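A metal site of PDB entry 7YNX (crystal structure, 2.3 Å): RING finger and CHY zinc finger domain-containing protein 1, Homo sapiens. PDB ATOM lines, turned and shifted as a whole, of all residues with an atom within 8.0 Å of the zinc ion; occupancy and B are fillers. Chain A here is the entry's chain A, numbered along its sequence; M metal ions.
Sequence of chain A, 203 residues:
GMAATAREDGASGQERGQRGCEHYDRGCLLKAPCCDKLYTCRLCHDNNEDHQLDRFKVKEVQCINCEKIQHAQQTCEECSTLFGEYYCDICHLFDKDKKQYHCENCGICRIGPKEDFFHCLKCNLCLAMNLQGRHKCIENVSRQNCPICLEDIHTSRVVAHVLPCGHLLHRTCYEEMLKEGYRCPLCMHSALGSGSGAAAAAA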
ATOM      1  N   GLY A  27     -13.034  25.333 -16.072  1.00  0.00           N
ATOM      2  CA  GLY A  27     -12.039  24.498 -16.683  1.00  0.00           C
ATOM      3  C   GLY A  27     -10.751  24.336 -15.920  1.00  0.00           C
ATOM      4  O   GLY A  27      -9.873  23.606 -16.359  1.00  0.00           O
ATOM      5  N   GLN A  62      -4.615  25.621 -12.522  1.00  0.00           N
ATOM      6  CA  GLN A  62      -4.182  24.454 -13.260  1.00  0.00           C
ATOM      7  C   GLN A  62      -5.282  24.017 -14.227  1.00  0.00           C
ATOM      8  O   GLN A  62      -6.426  23.807 -13.810  1.00  0.00           O
ATOM      9  CB  GLN A  62      -3.816  23.291 -12.317  1.00  0.00           C
ATOM     10  CG  GLN A  62      -3.551  21.981 -13.055  1.00  0.00           C
ATOM     11  CD  GLN A  62      -3.330  20.785 -12.113  1.00  0.00           C
ATOM     12  OE1 GLN A  62      -4.218  20.419 -11.344  1.00  0.00           O
ATOM     13  NE2 GLN A  62      -2.141  20.188 -12.176  1.00  0.00           N
ATOM     14  N   CYS A  63      -4.930  23.910 -15.498  1.00  0.00           N
ATOM     15  CA  CYS A  63      -5.880  23.400 -16.478  1.00  0.00           C
ATOM     16  C   CYS A  63      -6.267  21.973 -16.124  1.00  0.00           C
ATOM     17  O   CYS A  63      -5.395  21.129 -15.945  1.00  0.00           O
ATOM     18  CB  CYS A  63      -5.281  23.443 -17.884  1.00  0.00           C
ATOM     19  SG  CYS A  63      -6.329  22.664 -19.148  1.00  0.00           S
ATOM     20  N   ILE A  64      -7.572  21.726 -15.971  1.00  0.00           N
ATOM     21  CA  ILE A  64      -8.042  20.374 -15.719  1.00  0.00           C
ATOM     22  C   ILE A  64      -7.673  19.449 -16.878  1.00  0.00           C
ATOM     23  O   ILE A  64      -7.269  18.298 -16.687  1.00  0.00           O
ATOM     24  CB  ILE A  64      -9.571  20.377 -15.465  1.00  0.00           C
ATOM     25  CG1 ILE A  64      -9.938  21.341 -14.314  1.00  0.00           C
ATOM     26  CG2 ILE A  64     -10.067  18.970 -15.146  1.00  0.00           C
ATOM     27  CD1 ILE A  64     -11.320  21.061 -13.667  1.00  0.00           C
ATOM     28  N   ASN A  65      -7.774  19.970 -18.115  1.00  0.00           N
ATOM     29  CA  ASN A  65      -7.620  19.124 -19.302  1.00  0.00           C
ATOM     30  C   ASN A  65      -6.174  18.727 -19.554  1.00  0.00           C
ATOM     31  O   ASN A  65      -5.906  17.591 -19.957  1.00  0.00           O
ATOM     32  CB  ASN A  65      -8.192  19.855 -20.508  1.00  0.00           C
ATOM     33  CG  ASN A  65      -9.689  19.684 -20.628  1.00  0.00           C
ATOM     34  OD1 ASN A  65     -10.254  18.734 -20.106  1.00  0.00           O
ATOM     35  ND2 ASN A  65     -10.334  20.608 -21.332  1.00  0.00           N
ATOM     36  N   CYS A  66      -5.220  19.632 -19.363  1.00  0.00           N
ATOM     37  CA  CYS A  66      -3.831  19.313 -19.649  1.00  0.00           C
ATOM     38  C   CYS A  66      -2.900  19.551 -18.457  1.00  0.00           C
ATOM     39  O   CYS A  66      -1.678  19.404 -18.608  1.00  0.00           O
ATOM     40  CB  CYS A  66      -3.337  20.125 -20.839  1.00  0.00           C
ATOM     41  SG  CYS A  66      -2.740  21.709 -20.303  1.00  0.00           S
ATOM     42  N   GLU A  67      -3.437  19.904 -17.291  1.00  0.00           N
ATOM     43  CA  GLU A  67      -2.699  19.972 -16.039  1.00  0.00           C
ATOM     44  C   GLU A  67      -1.599  21.015 -16.070  1.00  0.00           C
ATOM     45  O   GLU A  67      -0.709  21.011 -15.212  1.00  0.00           O
ATOM     46  CB  GLU A  67      -2.146  18.599 -15.645  1.00  0.00           C
ATOM     47  CG  GLU A  67      -3.236  17.497 -15.599  1.00  0.00           C
ATOM     48  CD  GLU A  67      -2.786  16.185 -14.948  1.00  0.00           C
ATOM     49  OE1 GLU A  67      -1.754  16.164 -14.269  1.00  0.00           O
ATOM     50  OE2 GLU A  67      -3.489  15.166 -15.120  1.00  0.00           O
ATOM     51  N   LYS A  68      -1.639  21.940 -17.028  1.00  0.00           N
ATOM     52  CA  LYS A  68      -0.681  23.033 -17.062  1.00  0.00           C
ATOM     53  C   LYS A  68      -1.008  24.020 -15.932  1.00  0.00           C
ATOM     54  O   LYS A  68      -2.100  24.595 -15.900  1.00  0.00           O
ATOM     55  CB  LYS A  68      -0.708  23.728 -18.421  1.00  0.00           C
ATOM     56  CG  LYS A  68       0.346  24.792 -18.609  1.00  0.00           C
ATOM     57  CD  LYS A  68       1.659  24.389 -17.965  1.00  0.00           C
ATOM     58  CE  LYS A  68       2.800  25.265 -18.428  1.00  0.00           C
ATOM     59  NZ  LYS A  68       2.444  26.702 -18.325  1.00  0.00           N
ATOM     60  N   ILE A  69      -0.074  24.171 -15.006  1.00  0.00           N
ATOM     61  CA  ILE A  69      -0.213  25.154 -13.942  1.00  0.00           C
ATOM     62  C   ILE A  69       0.369  26.463 -14.460  1.00  0.00           C
ATOM     63  O   ILE A  69       1.439  26.471 -15.078  1.00  0.00           O
ATOM     64  CB  ILE A  69       0.492  24.677 -12.662  1.00  0.00           C
ATOM     65  CG1 ILE A  69      -0.126  23.361 -12.191  1.00  0.00           C
ATOM     66  CG2 ILE A  69       0.371  25.706 -11.569  1.00  0.00           C
ATOM     67  CD1 ILE A  69       0.569  22.761 -11.010  1.00  0.00           C
ATOM     68  N   GLN A  70      -0.359  27.559 -14.234  1.00  0.00           N
ATOM     69  CA  GLN A  70      -0.129  28.786 -14.992  1.00  0.00           C
ATOM     70  C   GLN A  70      -0.705  29.951 -14.210  1.00  0.00           C
ATOM     71  O   GLN A  70      -1.422  29.764 -13.221  1.00  0.00           O
ATOM     72  CB  GLN A  70      -0.770  28.709 -16.403  1.00  0.00           C
ATOM     73  CG  GLN A  70      -2.230  28.193 -16.404  1.00  0.00           C
ATOM     74  CD  GLN A  70      -2.802  27.921 -17.798  1.00  0.00           C
ATOM     75  OE1 GLN A  70      -3.025  28.840 -18.592  1.00  0.00           O
ATOM     76  NE2 GLN A  70      -3.048  26.644 -18.093  1.00  0.00           N
ATOM     77  N   THR A  75      -8.344  31.392 -20.721  1.00  0.00           N
ATOM     78  CA  THR A  75      -8.059  30.157 -21.437  1.00  0.00           C
ATOM     79  C   THR A  75      -6.651  29.685 -21.092  1.00  0.00           C
ATOM     80  O   THR A  75      -5.796  30.476 -20.694  1.00  0.00           O
ATOM     81  CB  THR A  75      -8.185  30.314 -22.947  1.00  0.00           C
ATOM     82  OG1 THR A  75      -7.393  31.435 -23.378  1.00  0.00           O
ATOM     83  CG2 THR A  75      -9.614  30.553 -23.338  1.00  0.00           C
ATOM     84  N   CYS A  76      -6.425  28.388 -21.298  1.00  0.00           N
ATOM     85  CA  CYS A  76      -5.142  27.767 -20.961  1.00  0.00           C
ATOM     86  C   CYS A  76      -4.043  28.192 -21.923  1.00  0.00           C
ATOM     87  O   CYS A  76      -4.192  28.094 -23.146  1.00  0.00           O
ATOM     88  CB  CYS A  76      -5.247  26.246 -20.968  1.00  0.00           C
ATOM     89  SG  CYS A  76      -3.607  25.457 -20.694  1.00  0.00           S
ATOM     90  N   GLU A  77      -2.910  28.603 -21.355  1.00  0.00           N
ATOM     91  CA  GLU A  77      -1.828  29.107 -22.191  1.00  0.00           C
ATOM     92  C   GLU A  77      -1.232  27.998 -23.048  1.00  0.00           C
ATOM     93  O   GLU A  77      -0.832  28.263 -24.190  1.00  0.00           O
ATOM     94  CB  GLU A  77      -0.750  29.770 -21.321  1.00  0.00           C
ATOM     95  CG  GLU A  77      -0.193  28.906 -20.218  1.00  0.00           C
ATOM     96  CD  GLU A  77       0.874  29.640 -19.402  1.00  0.00           C
ATOM     97  OE1 GLU A  77       0.651  30.814 -19.052  1.00  0.00           O
ATOM     98  OE2 GLU A  77       1.931  29.031 -19.124  1.00  0.00           O
ATOM     99  N   GLU A  78      -1.198  26.757 -22.563  1.00  0.00           N
ATOM    100  CA  GLU A  78      -0.705  25.659 -23.395  1.00  0.00           C
ATOM    101  C   GLU A  78      -1.771  25.149 -24.363  1.00  0.00           C
ATOM    102  O   GLU A  78      -1.594  25.216 -25.581  1.00  0.00           O
ATOM    103  CB  GLU A  78      -0.163  24.511 -22.524  1.00  0.00           C
ATOM    104  CG  GLU A  78       1.362  24.372 -22.551  1.00  0.00           C
ATOM    105  CD  GLU A  78       1.864  23.033 -22.011  1.00  0.00           C
ATOM    106  OE1 GLU A  78       3.021  22.970 -21.546  1.00  0.00           O
ATOM    107  OE2 GLU A  78       1.099  22.046 -22.052  1.00  0.00           O
ATOM    108  N   CYS A  79      -2.896  24.640 -23.847  1.00  0.00           N
ATOM    109  CA  CYS A  79      -3.816  23.881 -24.694  1.00  0.00           C
ATOM    110  C   CYS A  79      -5.092  24.628 -25.058  1.00  0.00           C
ATOM    111  O   CYS A  79      -5.897  24.083 -25.826  1.00  0.00           O
ATOM    112  CB  CYS A  79      -4.187  22.552 -24.015  1.00  0.00           C
ATOM    113  SG  CYS A  79      -5.541  22.712 -22.833  1.00  0.00           S
ATOM    114  N   SER A  80      -5.305  25.839 -24.532  1.00  0.00           N
ATOM    115  CA  SER A  80      -6.362  26.768 -24.940  1.00  0.00           C
ATOM    116  C   SER A  80      -7.760  26.333 -24.496  1.00  0.00           C
ATOM    117  O   SER A  80      -8.750  26.914 -24.934  1.00  0.00           O
ATOM    118  CB  SER A  80      -6.364  26.989 -26.453  1.00  0.00           C
ATOM    119  OG  SER A  80      -5.437  27.995 -26.802  1.00  0.00           O
ATOM    120  N   THR A  81      -7.868  25.309 -23.662  1.00  0.00           N
ATOM    121  CA  THR A  81      -9.156  24.969 -23.076  1.00  0.00           C
ATOM    122  C   THR A  81      -9.810  26.211 -22.476  1.00  0.00           C
ATOM    123  O   THR A  81      -9.123  27.058 -21.910  1.00  0.00           O
ATOM    124  CB  THR A  81      -8.935  23.868 -22.023  1.00  0.00           C
ATOM    125  OG1 THR A  81      -8.752  22.611 -22.683  1.00  0.00           O
ATOM    126  CG2 THR A  81     -10.088  23.772 -21.025  1.00  0.00           C
ATOM    127  N   LEU A  82     -11.120  26.339 -22.635  1.00  0.00           N
ATOM    128  CA  LEU A  82     -11.835  27.453 -22.030  1.00  0.00           C
ATOM    129  C   LEU A  82     -12.038  27.178 -20.542  1.00  0.00           C
ATOM    130  O   LEU A  82     -12.633  26.168 -20.165  1.00  0.00           O
ATOM    131  CB  LEU A  82     -13.182  27.675 -22.719  1.00  0.00           C
ATOM    132  CG  LEU A  82     -13.922  28.859 -22.083  1.00  0.00           C
ATOM    133  CD1 LEU A  82     -13.079  30.111 -22.169  1.00  0.00           C
ATOM    134  CD2 LEU A  82     -15.301  29.088 -22.698  1.00  0.00           C
ATOM    135  N   PHE A  83     -11.509  28.076 -19.689  1.00  0.00           N
ATOM    136  CA  PHE A  83     -11.582  27.897 -18.240  1.00  0.00           C
ATOM    137  C   PHE A  83     -12.932  28.325 -17.673  1.00  0.00           C
ATOM    138  O   PHE A  83     -13.480  27.642 -16.805  1.00  0.00           O
ATOM    139  CB  PHE A  83     -10.449  28.648 -17.564  1.00  0.00           C
ATOM    140  CG  PHE A  83      -9.133  27.960 -17.632  1.00  0.00           C
ATOM    141  CD1 PHE A  83      -9.056  26.640 -18.038  1.00  0.00           C
ATOM    142  CD2 PHE A  83      -7.983  28.623 -17.271  1.00  0.00           C
ATOM    143  CE1 PHE A  83      -7.834  26.001 -18.094  1.00  0.00           C
ATOM    144  CE2 PHE A  83      -6.746  27.984 -17.325  1.00  0.00           C
ATOM    145  CZ  PHE A  83      -6.675  26.672 -17.740  1.00  0.00           C
HETATM  146 ZN    ZN M   1      -4.512  23.281 -20.785  1.00  0.00          ZN
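The zinc ion is bound by SG of Cys 76 (2.4 Å), SG of Cys 79 (2.4 Å), SG of Cys 66 (2.4 Å) and SG of Cys 63 (2.5 Å). The zinc ion has four donor atoms within binding distance.
Four residues have an atom within 4 Å of the zinc ion: Cys 63, Cys 66, Cys 76 and Cys 79.
SG of Cys 76 lies close to NE2 of Gln 70 (2.9 Å). O of Thr 81 is in hydrogen-bond range of N of Cys 76, 3.1 Å away. SG of Cys 76 lies close to N of Glu 78, at 3.3 Å. SG of Cys 79 lies close to OG1 of Thr 81 (3.2 Å). The backbone NH (N) of Lys 68 sits close to the side-chain sulfur (SG) of Cys 66 (3.5 Å). The backbone NH (N) of Cys 63 lies within hydrogen-bond range of the backbone carbonyl oxygen (O) of Lys 68. The backbone NH of Asn 65 lies close to the side-chain sulfur of Cys 63, at 3.2 Å.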
